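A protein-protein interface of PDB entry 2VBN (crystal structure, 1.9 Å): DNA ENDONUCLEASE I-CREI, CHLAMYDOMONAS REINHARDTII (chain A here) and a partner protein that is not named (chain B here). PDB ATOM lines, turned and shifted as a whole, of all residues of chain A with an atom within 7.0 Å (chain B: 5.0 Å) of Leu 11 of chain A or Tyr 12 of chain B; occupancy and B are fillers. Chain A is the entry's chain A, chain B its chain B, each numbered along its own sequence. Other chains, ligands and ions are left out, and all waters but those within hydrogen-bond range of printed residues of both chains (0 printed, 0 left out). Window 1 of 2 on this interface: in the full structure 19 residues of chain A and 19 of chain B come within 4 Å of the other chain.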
ATOM      1  N   ASN A   6       6.152   9.146 -30.580  1.00  0.00           N
ATOM      2  CA  ASN A   6       5.023   9.966 -30.207  1.00  0.00           C
ATOM      3  C   ASN A   6       5.399  11.426 -30.013  1.00  0.00           C
ATOM      4  O   ASN A   6       6.546  11.746 -29.682  1.00  0.00           O
ATOM      5  CB  ASN A   6       4.372   9.395 -28.950  1.00  0.00           C
ATOM      6  CG  ASN A   6       3.725   8.033 -29.191  1.00  0.00           C
ATOM      7  OD1 ASN A   6       3.343   7.697 -30.321  1.00  0.00           O
ATOM      8  ND2 ASN A   6       3.626   7.231 -28.137  1.00  0.00           N
ATOM      9  N   LYS A   7       4.429  12.306 -30.243  1.00  0.00           N
ATOM     10  CA  LYS A   7       4.688  13.737 -30.335  1.00  0.00           C
ATOM     11  C   LYS A   7       5.258  14.315 -29.026  1.00  0.00           C
ATOM     12  O   LYS A   7       6.252  15.030 -29.035  1.00  0.00           O
ATOM     13  CB  LYS A   7       3.407  14.464 -30.798  1.00  0.00           C
ATOM     14  CG  LYS A   7       3.345  15.949 -30.515  1.00  0.00           C
ATOM     15  CD  LYS A   7       2.055  16.573 -31.039  1.00  0.00           C
ATOM     16  CE  LYS A   7       2.117  18.060 -30.823  1.00  0.00           C
ATOM     17  NZ  LYS A   7       0.969  18.796 -31.429  1.00  0.00           N
ATOM     18  N   GLU A   8       4.650  14.007 -27.893  1.00  0.00           N
ATOM     19  CA  GLU A   8       5.020  14.716 -26.647  1.00  0.00           C
ATOM     20  C   GLU A   8       6.387  14.240 -26.177  1.00  0.00           C
ATOM     21  O   GLU A   8       7.143  15.012 -25.602  1.00  0.00           O
ATOM     22  CB  GLU A   8       3.934  14.577 -25.571  1.00  0.00           C
ATOM     23  CG  GLU A   8       2.585  15.137 -26.129  1.00  0.00           C
ATOM     24  CD  GLU A   8       1.447  15.095 -25.145  1.00  0.00           C
ATOM     25  OE1 GLU A   8       1.521  14.248 -24.247  1.00  0.00           O
ATOM     26  OE2 GLU A   8       0.490  15.909 -25.259  1.00  0.00           O
ATOM     27  N   PHE A   9       6.694  12.976 -26.487  1.00  0.00           N
ATOM     28  CA  PHE A   9       8.011  12.383 -26.259  1.00  0.00           C
ATOM     29  C   PHE A   9       9.063  13.139 -27.079  1.00  0.00           C
ATOM     30  O   PHE A   9      10.027  13.626 -26.511  1.00  0.00           O
ATOM     31  CB  PHE A   9       7.987  10.888 -26.651  1.00  0.00           C
ATOM     32  CG  PHE A   9       9.354  10.269 -26.884  1.00  0.00           C
ATOM     33  CD1 PHE A   9      10.212  10.014 -25.827  1.00  0.00           C
ATOM     34  CD2 PHE A   9       9.762   9.912 -28.159  1.00  0.00           C
ATOM     35  CE1 PHE A   9      11.463   9.413 -26.044  1.00  0.00           C
ATOM     36  CE2 PHE A   9      11.013   9.333 -28.383  1.00  0.00           C
ATOM     37  CZ  PHE A   9      11.850   9.060 -27.320  1.00  0.00           C
ATOM     38  N   LEU A  10       8.853  13.250 -28.390  1.00  0.00           N
ATOM     39  CA  LEU A  10       9.771  13.966 -29.296  1.00  0.00           C
ATOM     40  C   LEU A  10       9.955  15.417 -28.895  1.00  0.00           C
ATOM     41  O   LEU A  10      11.059  15.981 -29.033  1.00  0.00           O
ATOM     42  CB  LEU A  10       9.292  13.911 -30.755  1.00  0.00           C
ATOM     43  CG  LEU A  10       9.308  12.498 -31.366  1.00  0.00           C
ATOM     44  CD1 LEU A  10       8.537  12.511 -32.665  1.00  0.00           C
ATOM     45  CD2 LEU A  10      10.752  12.047 -31.624  1.00  0.00           C
ATOM     46  N   LEU A  11       8.886  16.046 -28.413  1.00  0.00           N
ATOM     47  CA  LEU A  11       9.038  17.464 -28.041  1.00  0.00           C
ATOM     48  C   LEU A  11       9.944  17.619 -26.818  1.00  0.00           C
ATOM     49  O   LEU A  11      10.815  18.473 -26.798  1.00  0.00           O
ATOM     50  CB  LEU A  11       7.691  18.136 -27.771  1.00  0.00           C
ATOM     51  CG  LEU A  11       6.975  18.664 -29.011  1.00  0.00           C
ATOM     52  CD1 LEU A  11       5.490  18.744 -28.720  1.00  0.00           C
ATOM     53  CD2 LEU A  11       7.587  20.079 -29.113  1.00  0.00           C
ATOM     54  N   TYR A  12       9.666  16.847 -25.778  1.00  0.00           N
ATOM     55  CA  TYR A  12      10.463  16.907 -24.569  1.00  0.00           C
ATOM     56  C   TYR A  12      11.912  16.522 -24.925  1.00  0.00           C
ATOM     57  O   TYR A  12      12.871  17.171 -24.514  1.00  0.00           O
ATOM     58  CB  TYR A  12       9.931  15.948 -23.501  1.00  0.00           C
ATOM     59  CG  TYR A  12      10.908  15.822 -22.353  1.00  0.00           C
ATOM     60  CD1 TYR A  12      11.948  14.889 -22.384  1.00  0.00           C
ATOM     61  CD2 TYR A  12      10.817  16.676 -21.258  1.00  0.00           C
ATOM     62  CE1 TYR A  12      12.884  14.782 -21.318  1.00  0.00           C
ATOM     63  CE2 TYR A  12      11.735  16.602 -20.210  1.00  0.00           C
ATOM     64  CZ  TYR A  12      12.760  15.650 -20.247  1.00  0.00           C
ATOM     65  OH  TYR A  12      13.644  15.594 -19.210  1.00  0.00           O
ATOM     66  N   LEU A  13      12.070  15.473 -25.718  1.00  0.00           N
ATOM     67  CA  LEU A  13      13.398  14.908 -25.965  1.00  0.00           C
ATOM     68  C   LEU A  13      14.180  15.875 -26.819  1.00  0.00           C
ATOM     69  O   LEU A  13      15.377  16.045 -26.597  1.00  0.00           O
ATOM     70  CB  LEU A  13      13.338  13.518 -26.635  1.00  0.00           C
ATOM     71  CG  LEU A  13      14.724  12.931 -26.956  1.00  0.00           C
ATOM     72  CD1 LEU A  13      15.567  12.799 -25.636  1.00  0.00           C
ATOM     73  CD2 LEU A  13      14.543  11.566 -27.631  1.00  0.00           C
ATOM     74  N   ALA A  14      13.505  16.529 -27.768  1.00  0.00           N
ATOM     75  CA  ALA A  14      14.179  17.564 -28.570  1.00  0.00           C
ATOM     76  C   ALA A  14      14.823  18.636 -27.675  1.00  0.00           C
ATOM     77  O   ALA A  14      15.993  18.970 -27.871  1.00  0.00           O
ATOM     78  CB  ALA A  14      13.204  18.189 -29.578  1.00  0.00           C
ATOM     79  N   GLY A  15      14.049  19.184 -26.730  1.00  0.00           N
ATOM     80  CA  GLY A  15      14.542  20.086 -25.665  1.00  0.00           C
ATOM     81  C   GLY A  15      15.758  19.518 -24.946  1.00  0.00           C
ATOM     82  O   GLY A  15      16.824  20.161 -24.834  1.00  0.00           O
ATOM     83  N   PHE A  16      15.616  18.292 -24.472  1.00  0.00           N
ATOM     84  CA  PHE A  16      16.667  17.686 -23.665  1.00  0.00           C
ATOM     85  C   PHE A  16      17.945  17.486 -24.493  1.00  0.00           C
ATOM     86  O   PHE A  16      19.073  17.691 -23.998  1.00  0.00           O
ATOM     87  CB  PHE A  16      16.221  16.359 -23.043  1.00  0.00           C
ATOM     88  CG  PHE A  16      17.181  15.867 -21.983  1.00  0.00           C
ATOM     89  CD1 PHE A  16      17.111  16.390 -20.696  1.00  0.00           C
ATOM     90  CD2 PHE A  16      18.205  14.975 -22.294  1.00  0.00           C
ATOM     91  CE1 PHE A  16      17.986  15.984 -19.711  1.00  0.00           C
ATOM     92  CE2 PHE A  16      19.100  14.551 -21.300  1.00  0.00           C
ATOM     93  CZ  PHE A  16      18.984  15.066 -20.007  1.00  0.00           C
ATOM     94  N   VAL A  17      17.766  17.141 -25.765  1.00  0.00           N
ATOM     95  CA  VAL A  17      18.911  16.944 -26.656  1.00  0.00           C
ATOM     96  C   VAL A  17      19.578  18.285 -26.998  1.00  0.00           C
ATOM     97  O   VAL A  17      20.819  18.386 -27.056  1.00  0.00           O
ATOM     98  CB  VAL A  17      18.446  16.298 -27.967  1.00  0.00           C
ATOM     99  CG1 VAL A  17      19.558  16.438 -29.041  1.00  0.00           C
ATOM    100  CG2 VAL A  17      17.977  14.828 -27.691  1.00  0.00           C
ATOM    101  N   ASP A  18      18.775  19.318 -27.248  1.00  0.00           N
ATOM    102  CA  ASP A  18      19.349  20.642 -27.459  1.00  0.00           C
ATOM    103  C   ASP A  18      20.178  21.025 -26.228  1.00  0.00           C
ATOM    104  O   ASP A  18      21.154  21.773 -26.339  1.00  0.00           O
ATOM    105  CB  ASP A  18      18.241  21.697 -27.715  1.00  0.00           C
ATOM    106  CG  ASP A  18      17.871  21.839 -29.183  1.00  0.00           C
ATOM    107  OD1 ASP A  18      18.618  21.322 -30.048  1.00  0.00           O
ATOM    108  OD2 ASP A  18      16.823  22.470 -29.485  1.00  0.00           O
ATOM    109  N   GLY A  19      19.808  20.528 -25.048  1.00  0.00           N
ATOM    110  CA  GLY A  19      20.617  20.779 -23.829  1.00  0.00           C
ATOM    111  C   GLY A  19      21.842  19.878 -23.664  1.00  0.00           C
ATOM    112  O   GLY A  19      22.997  20.343 -23.780  1.00  0.00           O
ATOM    113  N   LEU A  91      12.679  13.471 -34.938  1.00  0.00           N
ATOM    114  CA  LEU A  91      13.087  14.454 -33.921  1.00  0.00           C
ATOM    115  C   LEU A  91      13.346  15.843 -34.508  1.00  0.00           C
ATOM    116  O   LEU A  91      13.018  16.854 -33.865  1.00  0.00           O
ATOM    117  CB  LEU A  91      14.349  13.979 -33.170  1.00  0.00           C
ATOM    118  CG  LEU A  91      14.839  14.818 -31.987  1.00  0.00           C
ATOM    119  CD1 LEU A  91      13.923  14.661 -30.777  1.00  0.00           C
ATOM    120  CD2 LEU A  91      16.295  14.424 -31.645  1.00  0.00           C
ATOM    121  N   PHE A  94      11.507  19.365 -34.225  1.00  0.00           N
ATOM    122  CA  PHE A  94      11.341  20.024 -32.929  1.00  0.00           C
ATOM    123  C   PHE A  94      12.641  20.571 -32.310  1.00  0.00           C
ATOM    124  O   PHE A  94      12.599  21.234 -31.277  1.00  0.00           O
ATOM    125  CB  PHE A  94      10.674  19.071 -31.930  1.00  0.00           C
ATOM    126  CG  PHE A  94       9.358  18.510 -32.420  1.00  0.00           C
ATOM    127  CD1 PHE A  94       8.248  19.328 -32.524  1.00  0.00           C
ATOM    128  CD2 PHE A  94       9.259  17.185 -32.810  1.00  0.00           C
ATOM    129  CE1 PHE A  94       7.022  18.829 -32.974  1.00  0.00           C
ATOM    130  CE2 PHE A  94       8.043  16.665 -33.233  1.00  0.00           C
ATOM    131  CZ  PHE A  94       6.922  17.509 -33.341  1.00  0.00           C
ATOM    132  N   LEU A  95      13.779  20.247 -32.905  1.00  0.00           N
ATOM    133  CA  LEU A  95      15.083  20.761 -32.490  1.00  0.00           C
ATOM    134  C   LEU A  95      15.246  22.252 -32.779  1.00  0.00           C
ATOM    135  O   LEU A  95      14.783  22.727 -33.817  1.00  0.00           O
ATOM    136  CB  LEU A  95      16.169  20.005 -33.273  1.00  0.00           C
ATOM    137  CG  LEU A  95      16.344  18.532 -32.822  1.00  0.00           C
ATOM    138  CD1 LEU A  95      17.356  17.820 -33.687  1.00  0.00           C
ATOM    139  CD2 LEU A  95      16.758  18.407 -31.324  1.00  0.00           C
ATOM    140  N   LYS A  96      15.921  22.992 -31.906  1.00  0.00           N
ATOM    141  CA  LYS A  96      16.103  24.449 -32.138  1.00  0.00           C
ATOM    142  C   LYS A  96      17.579  24.824 -32.270  1.00  0.00           C
ATOM    143  O   LYS A  96      17.966  25.662 -33.091  1.00  0.00           O
ATOM    144  CB  LYS A  96      15.521  25.260 -30.992  1.00  0.00           C
ATOM    145  CG  LYS A  96      13.991  25.175 -30.941  1.00  0.00           C
ATOM    146  CD  LYS A  96      13.382  26.060 -29.855  1.00  0.00           C
ATOM    147  CE  LYS A  96      11.855  25.878 -29.819  1.00  0.00           C
ATOM    148  NZ  LYS A  96      11.237  26.707 -28.751  1.00  0.00           N
ATOM    149  N   LEU A  97      18.407  24.231 -31.426  1.00  0.00           N
ATOM    150  CA  LEU A  97      19.858  24.447 -31.498  1.00  0.00           C
ATOM    151  C   LEU A  97      20.591  23.429 -32.349  1.00  0.00           C
ATOM    152  O   LEU A  97      21.633  23.749 -32.905  1.00  0.00           O
ATOM    153  CB  LEU A  97      20.445  24.375 -30.101  1.00  0.00           C
ATOM    154  CG  LEU A  97      19.920  25.508 -29.219  1.00  0.00           C
ATOM    155  CD1 LEU A  97      20.656  25.373 -27.838  1.00  0.00           C
ATOM    156  CD2 LEU A  97      20.191  26.867 -29.921  1.00  0.00           C
ATOM    157  N   LYS A  98      20.077  22.206 -32.453  1.00  0.00           N
ATOM    158  CA  LYS A  98      20.821  21.144 -33.164  1.00  0.00           C
ATOM    159  C   LYS A  98      20.098  20.649 -34.421  1.00  0.00           C
ATOM    160  O   LYS A  98      20.418  19.583 -34.961  1.00  0.00           O
ATOM    161  CB  LYS A  98      21.148  20.002 -32.198  1.00  0.00           C
ATOM    162  CG  LYS A  98      22.153  20.468 -31.089  1.00  0.00           C
ATOM    163  CD  LYS A  98      22.285  19.414 -30.008  1.00  0.00           C
ATOM    164  CE  LYS A  98      23.013  19.918 -28.751  1.00  0.00           C
ATOM    165  NZ  LYS A  98      24.444  19.895 -29.066  1.00  0.00           N
ATOM    166  N   GLU B   8       3.067  22.881 -26.148  1.00  0.00           N
ATOM    167  CA  GLU B   8       4.179  22.359 -26.940  1.00  0.00           C
ATOM    168  C   GLU B   8       5.462  23.114 -26.602  1.00  0.00           C
ATOM    169  O   GLU B   8       6.540  22.508 -26.519  1.00  0.00           O
ATOM    170  CB  GLU B   8       3.903  22.422 -28.451  1.00  0.00           C
ATOM    171  CG  GLU B   8       2.789  21.443 -28.916  1.00  0.00           C
ATOM    172  CD  GLU B   8       2.610  21.380 -30.422  1.00  0.00           C
ATOM    173  OE1 GLU B   8       3.568  21.733 -31.149  1.00  0.00           O
ATOM    174  OE2 GLU B   8       1.520  20.957 -30.885  1.00  0.00           O
ATOM    175  N   PHE B   9       5.345  24.416 -26.349  1.00  0.00           N
ATOM    176  CA  PHE B   9       6.495  25.193 -25.835  1.00  0.00           C
ATOM    177  C   PHE B   9       6.981  24.698 -24.473  1.00  0.00           C
ATOM    178  O   PHE B   9       8.203  24.532 -24.246  1.00  0.00           O
ATOM    179  CB  PHE B   9       6.145  26.695 -25.876  1.00  0.00           C
ATOM    180  CG  PHE B   9       6.996  27.556 -25.026  1.00  0.00           C
ATOM    181  CD1 PHE B   9       8.225  27.992 -25.471  1.00  0.00           C
ATOM    182  CD2 PHE B   9       6.557  27.956 -23.766  1.00  0.00           C
ATOM    183  CE1 PHE B   9       9.027  28.818 -24.651  1.00  0.00           C
ATOM    184  CE2 PHE B   9       7.348  28.777 -22.953  1.00  0.00           C
ATOM    185  CZ  PHE B   9       8.570  29.204 -23.398  1.00  0.00           C
ATOM    186  N   LEU B  10       6.045  24.441 -23.558  1.00  0.00           N
ATOM    187  CA  LEU B  10       6.378  23.920 -22.219  1.00  0.00           C
ATOM    188  C   LEU B  10       7.011  22.517 -22.262  1.00  0.00           C
ATOM    189  O   LEU B  10       7.946  22.212 -21.521  1.00  0.00           O
ATOM    190  CB  LEU B  10       5.130  23.869 -21.329  1.00  0.00           C
ATOM    191  CG  LEU B  10       4.478  25.197 -20.936  1.00  0.00           C
ATOM    192  CD1 LEU B  10       3.282  24.779 -20.127  1.00  0.00           C
ATOM    193  CD2 LEU B  10       5.453  26.042 -20.043  1.00  0.00           C
ATOM    194  N   LEU B  11       6.495  21.663 -23.138  1.00  0.00           N
ATOM    195  CA  LEU B  11       7.103  20.365 -23.330  1.00  0.00           C
ATOM    196  C   LEU B  11       8.576  20.503 -23.739  1.00  0.00           C
ATOM    197  O   LEU B  11       9.422  19.921 -23.084  1.00  0.00           O
ATOM    198  CB  LEU B  11       6.321  19.507 -24.341  1.00  0.00           C
ATOM    199  CG  LEU B  11       5.117  18.767 -23.755  1.00  0.00           C
ATOM    200  CD1 LEU B  11       4.177  18.391 -24.909  1.00  0.00           C
ATOM    201  CD2 LEU B  11       5.593  17.523 -22.978  1.00  0.00           C
ATOM    202  N   TYR B  12       8.865  21.236 -24.815  1.00  0.00           N
ATOM    203  CA  TYR B  12      10.230  21.443 -25.294  1.00  0.00           C
ATOM    204  C   TYR B  12      11.093  22.120 -24.208  1.00  0.00           C
ATOM    205  O   TYR B  12      12.203  21.671 -23.896  1.00  0.00           O
ATOM    206  CB  TYR B  12      10.230  22.309 -26.565  1.00  0.00           C
ATOM    207  CG  TYR B  12      11.621  22.723 -26.964  1.00  0.00           C
ATOM    208  CD1 TYR B  12      12.384  21.952 -27.863  1.00  0.00           C
ATOM    209  CD2 TYR B  12      12.221  23.838 -26.368  1.00  0.00           C
ATOM    210  CE1 TYR B  12      13.723  22.329 -28.187  1.00  0.00           C
ATOM    211  CE2 TYR B  12      13.521  24.227 -26.690  1.00  0.00           C
ATOM    212  CZ  TYR B  12      14.285  23.472 -27.576  1.00  0.00           C
ATOM    213  OH  TYR B  12      15.599  23.877 -27.830  1.00  0.00           O
ATOM    214  N   LEU B  13      10.571  23.191 -23.618  1.00  0.00           N
ATOM    215  CA  LEU B  13      11.319  23.911 -22.590  1.00  0.00           C
ATOM    216  C   LEU B  13      11.659  23.031 -21.363  1.00  0.00           C
ATOM    217  O   LEU B  13      12.753  23.109 -20.802  1.00  0.00           O
ATOM    218  CB  LEU B  13      10.606  25.211 -22.195  1.00  0.00           C
ATOM    219  CG  LEU B  13      11.365  26.113 -21.207  1.00  0.00           C
ATOM    220  CD1 LEU B  13      12.744  26.527 -21.719  1.00  0.00           C
ATOM    221  CD2 LEU B  13      10.518  27.340 -20.814  1.00  0.00           C
ATOM    222  N   ALA B  14      10.721  22.189 -20.954  1.00  0.00           N
ATOM    223  CA  ALA B  14      10.971  21.273 -19.824  1.00  0.00           C
ATOM    224  C   ALA B  14      12.191  20.378 -20.109  1.00  0.00           C
ATOM    225  O   ALA B  14      13.049  20.122 -19.220  1.00  0.00           O
ATOM    226  CB  ALA B  14       9.718  20.429 -19.543  1.00  0.00           C
ATOM    227  N   GLY B  15      12.278  19.908 -21.350  1.00  0.00           N
ATOM    228  CA  GLY B  15      13.419  19.094 -21.756  1.00  0.00           C
ATOM    229  C   GLY B  15      14.692  19.923 -21.711  1.00  0.00           C
ATOM    230  O   GLY B  15      15.719  19.485 -21.165  1.00  0.00           O
ATOM    231  N   PHE B  16      14.632  21.116 -22.298  1.00  0.00           N
ATOM    232  CA  PHE B  16      15.775  22.021 -22.289  1.00  0.00           C
ATOM    233  C   PHE B  16      16.239  22.382 -20.896  1.00  0.00           C
ATOM    234  O   PHE B  16      17.435  22.369 -20.606  1.00  0.00           O
ATOM    235  CB  PHE B  16      15.510  23.329 -23.056  1.00  0.00           C
ATOM    236  CG  PHE B  16      16.790  24.062 -23.410  1.00  0.00           C
ATOM    237  CD1 PHE B  16      17.628  23.541 -24.382  1.00  0.00           C
ATOM    238  CD2 PHE B  16      17.193  25.198 -22.722  1.00  0.00           C
ATOM    239  CE1 PHE B  16      18.844  24.141 -24.694  1.00  0.00           C
ATOM    240  CE2 PHE B  16      18.393  25.818 -23.043  1.00  0.00           C
ATOM    241  CZ  PHE B  16      19.219  25.291 -24.019  1.00  0.00           C
ATOM    242  N   PHE B  54      19.371  32.597 -28.076  1.00  0.00           N
ATOM    243  CA  PHE B  54      18.372  31.591 -27.700  1.00  0.00           C
ATOM    244  C   PHE B  54      17.778  31.970 -26.345  1.00  0.00           C
ATOM    245  O   PHE B  54      16.569  31.755 -26.104  1.00  0.00           O
ATOM    246  CB  PHE B  54      19.039  30.215 -27.634  1.00  0.00           C
ATOM    247  CG  PHE B  54      18.070  29.076 -27.497  1.00  0.00           C
ATOM    248  CD1 PHE B  54      17.950  28.378 -26.306  1.00  0.00           C
ATOM    249  CD2 PHE B  54      17.261  28.719 -28.555  1.00  0.00           C
ATOM    250  CE1 PHE B  54      17.073  27.290 -26.189  1.00  0.00           C
ATOM    251  CE2 PHE B  54      16.380  27.646 -28.431  1.00  0.00           C
ATOM    252  CZ  PHE B  54      16.297  26.930 -27.240  1.00  0.00           C
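NZ of Lys 7 of chain A lies within salt-bridge range of OE1 of Glu 8 of chain B (3.9 Å). The backbone NH (N) of Phe 16 of chain B lies close to the backbone carbonyl oxygen (O) of Gly 15 of chain A (3.5 Å). OH of Tyr 12 of chain B sits at hydrogen-bond distance from OD2 of Asp 18 of chain A, 2.5 Å away.
OD2 of Asp 18 of chain A is in hydrogen-bond range of N of Lys 96 of chain A, 2.6 Å away. The backbone NH (N) of Leu 97 of chain A lies within hydrogen-bond range of the side-chain carboxylate (OD2) of Asp 18 of chain A (3.1 Å). The backbone NH of Lys 98 of chain A sits at hydrogen-bond distance from the side-chain carboxylate of Asp 18 of chain A (2.9 Å).
Among the printed residues, pairs that only touch across the chains: Glu 8 of chain A with Leu 11 of chain B (3.8 Å), Leu 11 of chain A with Glu 8 of chain B (3.7 Å), Leu 11 of chain A with Leu 11 of chain B (3.9 Å), Leu 11 of chain A with Tyr 12 of chain B (3.4 Å), Tyr 12 of chain A with Leu 11 of chain B (3.5 Å), Tyr 12 of chain A with Ala 14 of chain B (3.8 Å), Tyr 12 of chain A with Gly 15 of chain B (3.4 Å), Ala 14 of chain A with Tyr 12 of chain B (3.9 Å), Gly 15 of chain A with Tyr 12 of chain B (3.3 Å), Gly 15 of chain A with Gly 15 of chain B (3.4 Å), Phe 16 of chain A with Gly 15 of chain B (3.2 Å), Phe 16 of chain A with Phe 16 of chain B (3.7 Å), Asp 18 of chain A with Phe 16 of chain B (3.7 Å), Gly 19 of chain A with Phe 16 of chain B (3.8 Å), Phe 94 of chain A with Tyr 12 of chain B (3.5 Å), Lys 96 of chain A with Tyr 12 of chain B (3.5 Å), Lys 96 of chain A with Phe 54 of chain B (3.6 Å), Leu 97 of chain A with Phe 16 of chain B (3.8 Å) and Leu 97 of chain A with Phe 54 of chain B (3.7 Å).
Leu 11 of chain A touches just these residues of chain B: Glu 8 (3.7 Å), Leu 11 (3.9 Å) and Tyr 12 (3.4 Å). Of chain A, only Leu 11, Ala 14, Gly 15, Asp 18, Phe 94 and Lys 96 come within 4 Å of Tyr 12 of chain B. Printed residues of chain A within 4 Å of Ala 14 of chain B: Tyr 12. Printed residues of chain A within 4 Å of Glu 8 of chain B: Lys 7 (2.3 Å) and Leu 11 (3.7 Å). Printed residues of chain B within 4 Å of Leu 97 of chain A: Phe 16 and Phe 54. Of the printed residues of chain B, Phe 94 of chain A touches Tyr 12. Of the printed residues of chain A, Phe 16 of chain B touches Gly 15, Phe 16, Asp 18, Gly 19 and Leu 97. Leu 10 of chain A touches none of the printed residues of chain B. Leu 95 of chain A touches none of the printed residues of chain B. The nearest printed residue of chain A that does not touch Tyr 12 of chain B is Tyr 12 of chain A (4.6 Å).
Of the 20 printed residues of chain A, 12 touch a printed residue of chain B. Printed residues of chain B that touch a printed residue of chain A: Glu 8, Leu 11, Tyr 12, Ala 14, Gly 15, Phe 16 and Phe 54.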
